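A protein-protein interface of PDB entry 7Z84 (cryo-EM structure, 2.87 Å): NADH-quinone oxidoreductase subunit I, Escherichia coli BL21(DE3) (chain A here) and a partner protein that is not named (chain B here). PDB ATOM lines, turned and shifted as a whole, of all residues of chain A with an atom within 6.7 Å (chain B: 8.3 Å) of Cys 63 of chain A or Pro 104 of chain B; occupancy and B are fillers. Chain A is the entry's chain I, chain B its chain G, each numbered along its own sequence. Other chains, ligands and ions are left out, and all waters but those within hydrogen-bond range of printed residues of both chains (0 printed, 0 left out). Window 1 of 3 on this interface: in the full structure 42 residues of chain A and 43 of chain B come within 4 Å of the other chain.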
ATOM      1  N   CYS A  60     -17.377  19.049  -2.524  1.00  0.00           N
ATOM      2  CA  CYS A  60     -17.671  19.415  -3.901  1.00  0.00           C
ATOM      3  C   CYS A  60     -16.945  18.499  -4.873  1.00  0.00           C
ATOM      4  O   CYS A  60     -15.733  18.295  -4.770  1.00  0.00           O
ATOM      5  CB  CYS A  60     -17.294  20.867  -4.172  1.00  0.00           C
ATOM      6  SG  CYS A  60     -17.553  21.344  -5.892  1.00  0.00           S
ATOM      7  N   VAL A  61     -17.701  17.947  -5.819  1.00  0.00           N
ATOM      8  CA  VAL A  61     -17.155  17.088  -6.856  1.00  0.00           C
ATOM      9  C   VAL A  61     -16.993  17.833  -8.176  1.00  0.00           C
ATOM     10  O   VAL A  61     -16.726  17.206  -9.204  1.00  0.00           O
ATOM     11  CB  VAL A  61     -18.019  15.832  -7.032  1.00  0.00           C
ATOM     12  CG1 VAL A  61     -18.155  15.106  -5.710  1.00  0.00           C
ATOM     13  CG2 VAL A  61     -19.387  16.200  -7.573  1.00  0.00           C
ATOM     14  N   ALA A  62     -17.155  19.161  -8.163  1.00  0.00           N
ATOM     15  CA  ALA A  62     -16.981  20.031  -9.330  1.00  0.00           C
ATOM     16  C   ALA A  62     -17.851  19.590 -10.506  1.00  0.00           C
ATOM     17  O   ALA A  62     -17.400  19.500 -11.648  1.00  0.00           O
ATOM     18  CB  ALA A  62     -15.510  20.124  -9.735  1.00  0.00           C
ATOM     19  N   CYS A  63     -19.113  19.306 -10.208  1.00  0.00           N
ATOM     20  CA  CYS A  63     -20.043  18.795 -11.202  1.00  0.00           C
ATOM     21  C   CYS A  63     -20.781  19.893 -11.957  1.00  0.00           C
ATOM     22  O   CYS A  63     -21.547  19.575 -12.874  1.00  0.00           O
ATOM     23  CB  CYS A  63     -21.045  17.859 -10.530  1.00  0.00           C
ATOM     24  SG  CYS A  63     -22.412  18.682  -9.718  1.00  0.00           S
ATOM     25  N   ASN A  64     -20.588  21.158 -11.574  1.00  0.00           N
ATOM     26  CA  ASN A  64     -21.081  22.343 -12.281  1.00  0.00           C
ATOM     27  C   ASN A  64     -22.604  22.415 -12.354  1.00  0.00           C
ATOM     28  O   ASN A  64     -23.145  23.094 -13.228  1.00  0.00           O
ATOM     29  CB  ASN A  64     -20.494  22.441 -13.696  1.00  0.00           C
ATOM     30  CG  ASN A  64     -19.303  23.370 -13.773  1.00  0.00           C
ATOM     31  OD1 ASN A  64     -19.442  24.586 -13.663  1.00  0.00           O
ATOM     32  ND2 ASN A  64     -18.125  22.801 -13.982  1.00  0.00           N
ATOM     33  N   LEU A  65     -23.321  21.731 -11.460  1.00  0.00           N
ATOM     34  CA  LEU A  65     -24.776  21.842 -11.459  1.00  0.00           C
ATOM     35  C   LEU A  65     -25.231  23.162 -10.849  1.00  0.00           C
ATOM     36  O   LEU A  65     -26.225  23.747 -11.294  1.00  0.00           O
ATOM     37  CB  LEU A  65     -25.397  20.668 -10.703  1.00  0.00           C
ATOM     38  CG  LEU A  65     -25.587  19.352 -11.459  1.00  0.00           C
ATOM     39  CD1 LEU A  65     -26.240  18.319 -10.557  1.00  0.00           C
ATOM     40  CD2 LEU A  65     -26.395  19.543 -12.732  1.00  0.00           C
ATOM     41  N   CYS A  66     -24.516  23.642  -9.831  1.00  0.00           N
ATOM     42  CA  CYS A  66     -24.860  24.910  -9.199  1.00  0.00           C
ATOM     43  C   CYS A  66     -24.618  26.086 -10.135  1.00  0.00           C
ATOM     44  O   CYS A  66     -25.365  27.070 -10.107  1.00  0.00           O
ATOM     45  CB  CYS A  66     -24.055  25.084  -7.916  1.00  0.00           C
ATOM     46  SG  CYS A  66     -22.275  24.995  -8.145  1.00  0.00           S
ATOM     47  N   VAL A  68     -24.815  26.105 -13.457  1.00  0.00           N
ATOM     48  CA  VAL A  68     -25.824  26.162 -14.508  1.00  0.00           C
ATOM     49  C   VAL A  68     -27.209  26.415 -13.923  1.00  0.00           C
ATOM     50  O   VAL A  68     -28.065  27.014 -14.583  1.00  0.00           O
ATOM     51  CB  VAL A  68     -25.762  24.882 -15.366  1.00  0.00           C
ATOM     52  CG1 VAL A  68     -26.103  23.651 -14.554  1.00  0.00           C
ATOM     53  CG2 VAL A  68     -26.644  24.992 -16.606  1.00  0.00           C
ATOM     54  N   LEU A  77     -16.327  27.619 -11.861  1.00  0.00           N
ATOM     55  CA  LEU A  77     -15.506  26.574 -11.271  1.00  0.00           C
ATOM     56  C   LEU A  77     -14.898  25.728 -12.380  1.00  0.00           C
ATOM     57  O   LEU A  77     -15.317  25.794 -13.537  1.00  0.00           O
ATOM     58  CB  LEU A  77     -16.323  25.707 -10.306  1.00  0.00           C
ATOM     59  CG  LEU A  77     -17.431  24.862 -10.937  1.00  0.00           C
ATOM     60  CD1 LEU A  77     -17.096  23.395 -10.822  1.00  0.00           C
ATOM     61  CD2 LEU A  77     -18.776  25.157 -10.305  1.00  0.00           C
ATOM     62  N   LYS A  79     -13.246  21.613 -12.914  1.00  0.00           N
ATOM     63  CA  LYS A  79     -12.986  20.292 -12.363  1.00  0.00           C
ATOM     64  C   LYS A  79     -11.502  19.949 -12.425  1.00  0.00           C
ATOM     65  O   LYS A  79     -10.837  20.173 -13.439  1.00  0.00           O
ATOM     66  CB  LYS A  79     -13.805  19.243 -13.120  1.00  0.00           C
ATOM     67  CG  LYS A  79     -13.524  17.805 -12.722  1.00  0.00           C
ATOM     68  CD  LYS A  79     -12.857  17.052 -13.855  1.00  0.00           C
ATOM     69  CE  LYS A  79     -12.173  15.795 -13.366  1.00  0.00           C
ATOM     70  NZ  LYS A  79     -11.583  15.027 -14.492  1.00  0.00           N
ATOM     71  N   TRP A  87     -12.963  13.719  -7.789  1.00  0.00           N
ATOM     72  CA  TRP A  87     -13.179  15.006  -8.429  1.00  0.00           C
ATOM     73  C   TRP A  87     -13.264  16.101  -7.375  1.00  0.00           C
ATOM     74  O   TRP A  87     -13.873  15.913  -6.320  1.00  0.00           O
ATOM     75  CB  TRP A  87     -14.465  14.987  -9.253  1.00  0.00           C
ATOM     76  CG  TRP A  87     -14.405  14.223 -10.538  1.00  0.00           C
ATOM     77  CD1 TRP A  87     -13.590  13.174 -10.837  1.00  0.00           C
ATOM     78  CD2 TRP A  87     -15.220  14.440 -11.694  1.00  0.00           C
ATOM     79  NE1 TRP A  87     -13.838  12.731 -12.112  1.00  0.00           N
ATOM     80  CE2 TRP A  87     -14.835  13.494 -12.660  1.00  0.00           C
ATOM     81  CE3 TRP A  87     -16.231  15.352 -12.009  1.00  0.00           C
ATOM     82  CZ2 TRP A  87     -15.428  13.428 -13.916  1.00  0.00           C
ATOM     83  CZ3 TRP A  87     -16.818  15.287 -13.257  1.00  0.00           C
ATOM     84  CH2 TRP A  87     -16.416  14.333 -14.195  1.00  0.00           C
ATOM     85  N   ALA A 108     -29.687  22.670  -6.040  1.00  0.00           N
ATOM     86  CA  ALA A 108     -29.206  21.852  -7.143  1.00  0.00           C
ATOM     87  C   ALA A 108     -28.000  20.992  -6.791  1.00  0.00           C
ATOM     88  O   ALA A 108     -27.609  20.153  -7.607  1.00  0.00           O
ATOM     89  CB  ALA A 108     -28.855  22.732  -8.340  1.00  0.00           C
ATOM     90  N   CYS A 109     -27.406  21.169  -5.620  1.00  0.00           N
ATOM     91  CA  CYS A 109     -26.192  20.432  -5.287  1.00  0.00           C
ATOM     92  C   CYS A 109     -26.519  18.986  -4.952  1.00  0.00           C
ATOM     93  O   CYS A 109     -27.291  18.735  -4.019  1.00  0.00           O
ATOM     94  CB  CYS A 109     -25.463  21.082  -4.121  1.00  0.00           C
ATOM     95  SG  CYS A 109     -23.796  20.430  -3.811  1.00  0.00           S
ATOM     96  N   PRO A 110     -25.959  18.012  -5.666  1.00  0.00           N
ATOM     97  CA  PRO A 110     -26.199  16.602  -5.347  1.00  0.00           C
ATOM     98  C   PRO A 110     -25.242  16.020  -4.320  1.00  0.00           C
ATOM     99  O   PRO A 110     -25.330  14.824  -4.028  1.00  0.00           O
ATOM    100  CB  PRO A 110     -26.001  15.931  -6.710  1.00  0.00           C
ATOM    101  CG  PRO A 110     -24.976  16.776  -7.372  1.00  0.00           C
ATOM    102  CD  PRO A 110     -25.124  18.173  -6.867  1.00  0.00           C
ATOM    103  N   THR A 111     -24.321  16.822  -3.789  1.00  0.00           N
ATOM    104  CA  THR A 111     -23.413  16.385  -2.742  1.00  0.00           C
ATOM    105  C   THR A 111     -23.570  17.181  -1.456  1.00  0.00           C
ATOM    106  O   THR A 111     -22.859  16.895  -0.488  1.00  0.00           O
ATOM    107  CB  THR A 111     -21.953  16.476  -3.210  1.00  0.00           C
ATOM    108  OG1 THR A 111     -21.495  17.826  -3.089  1.00  0.00           O
ATOM    109  CG2 THR A 111     -21.805  16.027  -4.653  1.00  0.00           C
ATOM    110  N   PHE A 150     -21.311  12.031  -0.590  1.00  0.00           N
ATOM    111  CA  PHE A 150     -21.662  11.575  -1.931  1.00  0.00           C
ATOM    112  C   PHE A 150     -20.790  10.407  -2.370  1.00  0.00           C
ATOM    113  O   PHE A 150     -21.268   9.492  -3.049  1.00  0.00           O
ATOM    114  CB  PHE A 150     -21.550  12.725  -2.929  1.00  0.00           C
ATOM    115  CG  PHE A 150     -21.635  12.289  -4.363  1.00  0.00           C
ATOM    116  CD1 PHE A 150     -22.845  11.905  -4.912  1.00  0.00           C
ATOM    117  CD2 PHE A 150     -20.502  12.257  -5.161  1.00  0.00           C
ATOM    118  CE1 PHE A 150     -22.923  11.496  -6.227  1.00  0.00           C
ATOM    119  CE2 PHE A 150     -20.576  11.850  -6.473  1.00  0.00           C
ATOM    120  CZ  PHE A 150     -21.786  11.469  -7.007  1.00  0.00           C
ATOM    121  N   PRO B 100     -24.699   2.862 -11.251  1.00  0.00           N
ATOM    122  CA  PRO B 100     -24.082   3.552 -10.117  1.00  0.00           C
ATOM    123  C   PRO B 100     -24.601   4.972  -9.973  1.00  0.00           C
ATOM    124  O   PRO B 100     -25.009   5.614 -10.941  1.00  0.00           O
ATOM    125  CB  PRO B 100     -22.593   3.542 -10.471  1.00  0.00           C
ATOM    126  CG  PRO B 100     -22.580   3.531 -11.951  1.00  0.00           C
ATOM    127  CD  PRO B 100     -23.758   2.702 -12.372  1.00  0.00           C
ATOM    128  N   HIS B 101     -24.563   5.464  -8.734  1.00  0.00           N
ATOM    129  CA  HIS B 101     -24.983   6.825  -8.399  1.00  0.00           C
ATOM    130  C   HIS B 101     -23.856   7.792  -8.766  1.00  0.00           C
ATOM    131  O   HIS B 101     -23.213   8.415  -7.919  1.00  0.00           O
ATOM    132  CB  HIS B 101     -25.340   6.894  -6.920  1.00  0.00           C
ATOM    133  CG  HIS B 101     -26.053   8.144  -6.518  1.00  0.00           C
ATOM    134  ND1 HIS B 101     -27.425   8.260  -6.556  1.00  0.00           N
ATOM    135  CD2 HIS B 101     -25.589   9.324  -6.045  1.00  0.00           C
ATOM    136  CE1 HIS B 101     -27.774   9.463  -6.137  1.00  0.00           C
ATOM    137  NE2 HIS B 101     -26.678  10.129  -5.822  1.00  0.00           N
ATOM    138  N   ASP B 102     -23.632   7.927 -10.074  1.00  0.00           N
ATOM    139  CA  ASP B 102     -22.371   8.441 -10.588  1.00  0.00           C
ATOM    140  C   ASP B 102     -22.479   9.699 -11.435  1.00  0.00           C
ATOM    141  O   ASP B 102     -21.437  10.214 -11.851  1.00  0.00           O
ATOM    142  CB  ASP B 102     -21.667   7.359 -11.417  1.00  0.00           C
ATOM    143  CG  ASP B 102     -20.501   6.736 -10.697  1.00  0.00           C
ATOM    144  OD1 ASP B 102     -20.396   6.917  -9.468  1.00  0.00           O
ATOM    145  OD2 ASP B 102     -19.685   6.068 -11.362  1.00  0.00           O
ATOM    146  N   CYS B 103     -23.686  10.204 -11.702  1.00  0.00           N
ATOM    147  CA  CYS B 103     -23.868  11.327 -12.625  1.00  0.00           C
ATOM    148  C   CYS B 103     -23.065  12.593 -12.307  1.00  0.00           C
ATOM    149  O   CYS B 103     -22.571  13.214 -13.263  1.00  0.00           O
ATOM    150  CB  CYS B 103     -25.359  11.683 -12.738  1.00  0.00           C
ATOM    151  SG  CYS B 103     -26.437  10.418 -13.424  1.00  0.00           S
ATOM    152  N   PRO B 104     -22.918  13.054 -11.051  1.00  0.00           N
ATOM    153  CA  PRO B 104     -22.035  14.213 -10.818  1.00  0.00           C
ATOM    154  C   PRO B 104     -20.574  13.978 -11.170  1.00  0.00           C
ATOM    155  O   PRO B 104     -19.889  14.924 -11.574  1.00  0.00           O
ATOM    156  CB  PRO B 104     -22.204  14.481  -9.318  1.00  0.00           C
ATOM    157  CG  PRO B 104     -23.517  13.944  -8.999  1.00  0.00           C
ATOM    158  CD  PRO B 104     -23.656  12.722  -9.815  1.00  0.00           C
ATOM    159  N   VAL B 105     -20.074  12.752 -11.039  1.00  0.00           N
ATOM    160  CA  VAL B 105     -18.658  12.480 -11.254  1.00  0.00           C
ATOM    161  C   VAL B 105     -18.472  11.683 -12.535  1.00  0.00           C
ATOM    162  O   VAL B 105     -17.537  10.885 -12.655  1.00  0.00           O
ATOM    163  CB  VAL B 105     -18.044  11.735 -10.058  1.00  0.00           C
ATOM    164  CG1 VAL B 105     -17.741  12.700  -8.938  1.00  0.00           C
ATOM    165  CG2 VAL B 105     -18.976  10.637  -9.581  1.00  0.00           C
ATOM    166  N   CYS B 106     -19.361  11.894 -13.499  1.00  0.00           N
ATOM    167  CA  CYS B 106     -19.347  11.180 -14.767  1.00  0.00           C
ATOM    168  C   CYS B 106     -19.217  12.181 -15.902  1.00  0.00           C
ATOM    169  O   CYS B 106     -19.938  13.182 -15.936  1.00  0.00           O
ATOM    170  CB  CYS B 106     -20.617  10.353 -14.925  1.00  0.00           C
ATOM    171  SG  CYS B 106     -20.805   9.452 -16.449  1.00  0.00           S
ATOM    172  N   GLU B 107     -18.305  11.902 -16.832  1.00  0.00           N
ATOM    173  CA  GLU B 107     -18.058  12.809 -17.945  1.00  0.00           C
ATOM    174  C   GLU B 107     -19.192  12.828 -18.960  1.00  0.00           C
ATOM    175  O   GLU B 107     -19.226  13.728 -19.804  1.00  0.00           O
ATOM    176  CB  GLU B 107     -16.747  12.440 -18.638  1.00  0.00           C
ATOM    177  CG  GLU B 107     -15.509  12.642 -17.778  1.00  0.00           C
ATOM    178  CD  GLU B 107     -15.155  11.417 -16.954  1.00  0.00           C
ATOM    179  OE1 GLU B 107     -15.953  10.456 -16.933  1.00  0.00           O
ATOM    180  OE2 GLU B 107     -14.076  11.413 -16.325  1.00  0.00           O
ATOM    181  N   GLU B 108     -20.114  11.867 -18.902  1.00  0.00           N
ATOM    182  CA  GLU B 108     -21.261  11.847 -19.797  1.00  0.00           C
ATOM    183  C   GLU B 108     -22.438  12.663 -19.272  1.00  0.00           C
ATOM    184  O   GLU B 108     -23.414  12.841 -20.004  1.00  0.00           O
ATOM    185  CB  GLU B 108     -21.691  10.396 -20.048  1.00  0.00           C
ATOM    186  CG  GLU B 108     -22.410  10.143 -21.372  1.00  0.00           C
ATOM    187  CD  GLU B 108     -21.470   9.887 -22.538  1.00  0.00           C
ATOM    188  OE1 GLU B 108     -20.257  10.148 -22.410  1.00  0.00           O
ATOM    189  OE2 GLU B 108     -21.954   9.426 -23.592  1.00  0.00           O
ATOM    190  N   GLY B 109     -22.365  13.170 -18.041  1.00  0.00           N
ATOM    191  CA  GLY B 109     -23.447  13.934 -17.443  1.00  0.00           C
ATOM    192  C   GLY B 109     -23.834  15.188 -18.199  1.00  0.00           C
ATOM    193  O   GLY B 109     -22.981  16.014 -18.531  1.00  0.00           O
ATOM    194  N   GLY B 110     -25.127  15.335 -18.486  1.00  0.00           N
ATOM    195  CA  GLY B 110     -25.615  16.398 -19.338  1.00  0.00           C
ATOM    196  C   GLY B 110     -25.446  16.146 -20.816  1.00  0.00           C
ATOM    197  O   GLY B 110     -25.950  16.931 -21.628  1.00  0.00           O
ATOM    198  N   GLN B 115     -29.519   9.296 -19.593  1.00  0.00           N
ATOM    199  CA  GLN B 115     -30.218  10.331 -18.835  1.00  0.00           C
ATOM    200  C   GLN B 115     -31.448  10.827 -19.586  1.00  0.00           C
ATOM    201  O   GLN B 115     -32.537  10.963 -19.008  1.00  0.00           O
ATOM    202  CB  GLN B 115     -29.273  11.500 -18.551  1.00  0.00           C
ATOM    203  CG  GLN B 115     -28.492  11.400 -17.262  1.00  0.00           C
ATOM    204  CD  GLN B 115     -27.518  12.546 -17.095  1.00  0.00           C
ATOM    205  OE1 GLN B 115     -27.058  13.128 -18.075  1.00  0.00           O
ATOM    206  NE2 GLN B 115     -27.199  12.877 -15.853  1.00  0.00           N
ATOM    207  N   ARG B 150     -21.159   1.732 -15.475  1.00  0.00           N
ATOM    208  CA  ARG B 150     -22.231   2.494 -16.097  1.00  0.00           C
ATOM    209  C   ARG B 150     -22.829   1.805 -17.315  1.00  0.00           C
ATOM    210  O   ARG B 150     -23.705   2.384 -17.964  1.00  0.00           O
ATOM    211  CB  ARG B 150     -21.716   3.881 -16.489  1.00  0.00           C
ATOM    212  CG  ARG B 150     -21.270   4.717 -15.305  1.00  0.00           C
ATOM    213  CD  ARG B 150     -20.332   5.819 -15.735  1.00  0.00           C
ATOM    214  NE  ARG B 150     -19.685   6.454 -14.596  1.00  0.00           N
ATOM    215  CZ  ARG B 150     -18.604   7.215 -14.680  1.00  0.00           C
ATOM    216  NH1 ARG B 150     -18.012   7.448 -15.839  1.00  0.00           N
ATOM    217  NH2 ARG B 150     -18.099   7.750 -13.572  1.00  0.00           N
ATOM    218  N   TYR B 215     -12.039  18.857 -17.832  1.00  0.00           N
ATOM    219  CA  TYR B 215     -13.426  18.539 -18.136  1.00  0.00           C
ATOM    220  C   TYR B 215     -14.355  19.709 -17.847  1.00  0.00           C
ATOM    221  O   TYR B 215     -14.227  20.396 -16.831  1.00  0.00           O
ATOM    222  CB  TYR B 215     -13.890  17.312 -17.350  1.00  0.00           C
ATOM    223  CG  TYR B 215     -15.340  16.972 -17.609  1.00  0.00           C
ATOM    224  CD1 TYR B 215     -15.729  16.397 -18.811  1.00  0.00           C
ATOM    225  CD2 TYR B 215     -16.321  17.240 -16.664  1.00  0.00           C
ATOM    226  CE1 TYR B 215     -17.049  16.099 -19.063  1.00  0.00           C
ATOM    227  CE2 TYR B 215     -17.644  16.944 -16.908  1.00  0.00           C
ATOM    228  CZ  TYR B 215     -18.001  16.371 -18.108  1.00  0.00           C
ATOM    229  OH  TYR B 215     -19.319  16.071 -18.355  1.00  0.00           O
ATOM    230  N   ASN B 216     -15.299  19.924 -18.759  1.00  0.00           N
ATOM    231  CA  ASN B 216     -16.417  20.825 -18.542  1.00  0.00           C
ATOM    232  C   ASN B 216     -17.636  20.225 -19.224  1.00  0.00           C
ATOM    233  O   ASN B 216     -17.516  19.423 -20.152  1.00  0.00           O
ATOM    234  CB  ASN B 216     -16.134  22.233 -19.076  1.00  0.00           C
ATOM    235  CG  ASN B 216     -16.298  22.328 -20.576  1.00  0.00           C
ATOM    236  OD1 ASN B 216     -17.211  22.988 -21.068  1.00  0.00           O
ATOM    237  ND2 ASN B 216     -15.412  21.674 -21.313  1.00  0.00           N
ATOM    238  N   ARG B 217     -18.812  20.619 -18.751  1.00  0.00           N
ATOM    239  CA  ARG B 217     -20.056  20.052 -19.243  1.00  0.00           C
ATOM    240  C   ARG B 217     -20.397  20.609 -20.625  1.00  0.00           C
ATOM    241  O   ARG B 217     -19.804  21.581 -21.097  1.00  0.00           O
ATOM    242  CB  ARG B 217     -21.185  20.324 -18.256  1.00  0.00           C
ATOM    243  CG  ARG B 217     -20.914  19.789 -16.862  1.00  0.00           C
ATOM    244  CD  ARG B 217     -21.393  18.359 -16.709  1.00  0.00           C
ATOM    245  NE  ARG B 217     -21.186  17.859 -15.357  1.00  0.00           N
ATOM    246  CZ  ARG B 217     -20.991  16.584 -15.052  1.00  0.00           C
ATOM    247  NH1 ARG B 217     -20.958  15.650 -15.985  1.00  0.00           N
ATOM    248  NH2 ARG B 217     -20.817  16.239 -13.781  1.00  0.00           N
ATOM    249  N   TRP B 219     -23.203  22.053 -21.721  1.00  0.00           N
ATOM    250  CA  TRP B 219     -23.870  23.348 -21.712  1.00  0.00           C
ATOM    251  C   TRP B 219     -22.904  24.506 -21.486  1.00  0.00           C
ATOM    252  O   TRP B 219     -23.244  25.650 -21.799  1.00  0.00           O
ATOM    253  CB  TRP B 219     -24.973  23.364 -20.648  1.00  0.00           C
ATOM    254  CG  TRP B 219     -24.507  23.056 -19.250  1.00  0.00           C
ATOM    255  CD1 TRP B 219     -23.803  23.878 -18.419  1.00  0.00           C
ATOM    256  CD2 TRP B 219     -24.722  21.843 -18.520  1.00  0.00           C
ATOM    257  NE1 TRP B 219     -23.558  23.251 -17.226  1.00  0.00           N
ATOM    258  CE2 TRP B 219     -24.119  22.002 -17.258  1.00  0.00           C
ATOM    259  CE3 TRP B 219     -25.364  20.636 -18.813  1.00  0.00           C
ATOM    260  CZ2 TRP B 219     -24.143  21.005 -16.288  1.00  0.00           C
ATOM    261  CZ3 TRP B 219     -25.378  19.646 -17.852  1.00  0.00           C
ATOM    262  CH2 TRP B 219     -24.771  19.834 -16.606  1.00  0.00           C
ATOM    263  N   ASP B 220     -21.718  24.236 -20.952  1.00  0.00           N
ATOM    264  CA  ASP B 220     -20.715  25.262 -20.709  1.00  0.00           C
ATOM    265  C   ASP B 220     -19.767  25.457 -21.883  1.00  0.00           C
ATOM    266  O   ASP B 220     -18.862  26.287 -21.795  1.00  0.00           O
ATOM    267  CB  ASP B 220     -19.907  24.918 -19.455  1.00  0.00           C
ATOM    268  CG  ASP B 220     -20.593  25.359 -18.185  1.00  0.00           C
ATOM    269  OD1 ASP B 220     -21.541  26.166 -18.271  1.00  0.00           O
ATOM    270  OD2 ASP B 220     -20.190  24.895 -17.099  1.00  0.00           O
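The guanidinium group of Arg 217 of chain B sits at hydrogen-bond distance from the backbone carbonyl oxygen of Cys 63 of chain A (3.0 Å).
The guanidinium group (NH1) of Arg 150 of chain B is in salt-bridge range of the side-chain carboxylate (OE1) of Glu 107 of chain B (3.8 Å). The side-chain sulfur (SG) of Cys 106 of chain B lies close to the backbone NH (N) of Glu 108 of chain B, at 3.5 Å. O of Cys 106 of chain B is in hydrogen-bond range of NH1 of Arg 217 of chain B (2.7 Å). NH1 of Arg 217 of chain B sits at hydrogen-bond distance from OH of Tyr 215 of chain B (2.9 Å). The guanidinium group (NH2) of Arg 217 of chain B is in hydrogen-bond range of the backbone carbonyl oxygen (O) of Pro 104 of chain B (2.7 Å). O of Gly 109 of chain B lies within hydrogen-bond range of NH1 of Arg 217 of chain B, 3.3 Å away.
Among the printed residues, pairs that only touch across the chains: Val 68 of chain A with Trp 219 of chain B (3.3 Å), Cys 63 of chain A with Pro 104 of chain B (3.3 Å), Trp 87 of chain A with Glu 107 of chain B (3.4 Å), Phe 150 of chain A with His 101 of chain B (3.4 Å), Trp 87 of chain A with Pro 104 of chain B (3.5 Å), Asn 64 of chain A with Asp 220 of chain B (3.5 Å), Trp 87 of chain A with Val 105 of chain B (3.5 Å), Pro 110 of chain A with Pro 104 of chain B (3.6 Å), Phe 150 of chain A with Pro 104 of chain B (3.6 Å), Lys 79 of chain A with Tyr 215 of chain B (3.7 Å), Val 61 of chain A with Val 105 of chain B (3.7 Å), Phe 150 of chain A with Val 105 of chain B (3.7 Å), Val 61 of chain A with Pro 104 of chain B (3.7 Å), Trp 87 of chain A with Tyr 215 of chain B (3.8 Å), Asn 64 of chain A with Trp 219 of chain B (3.8 Å) and Trp 87 of chain A with Cys 106 of chain B (3.9 Å).
Printed residues of chain B within 4 Å of Val 61 of chain A: Pro 104 and Val 105. Cys 63 of chain A touches just these residues of chain B: Pro 104 (3.3 Å) and Arg 217 (3.0 Å). Leu 65 of chain A touches none of the printed residues of chain B. Of the printed residues of chain B, Lys 79 of chain A touches Tyr 215. Of the printed residues of chain B, Pro 110 of chain A touches Pro 104. Of the printed residues of chain B, Phe 150 of chain A touches His 101 (3.4 Å), Pro 104 (3.6 Å) and Val 105 (3.7 Å). Of the printed residues of chain A, Pro 104 of chain B touches Val 61 (3.7 Å), Cys 63 (3.3 Å), Trp 87 (3.5 Å), Pro 110 (3.6 Å) and Phe 150 (3.6 Å). Arg 150 of chain B touches none of the printed residues of chain A. The nearest residue of chain B that does not touch Cys 63 of chain A is Trp 219 of chain B (4.5 Å). The nearest residue of chain A that does not touch Pro 104 of chain B is Thr 111 of chain A (4.9 Å).
Hydrophobic or aromatic side chains of chain A within 4 Å of the printed part of chain B: Val 61, Val 68, Trp 87, Pro 110 and Phe 150. Of the 18 printed residues of chain B, 9 touch a printed residue of chain A. Printed residues of chain B that touch a printed residue of chain A: His 101, Pro 104, Val 105, Cys 106, Glu 107, Tyr 215, Arg 217, Trp 219 and Asp 220. Hydrophobic or aromatic side chains of chain B within 4 Å of the printed part of chain A: His 101, Pro 104, Val 105, Tyr 215 and Trp 219. Among the printed residues, 17 pairs touch across the chains. Among the printed residues, no Asp or Glu carboxylate lies within 4 Å of a Lys or Arg side-chain nitrogen of the other chain.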
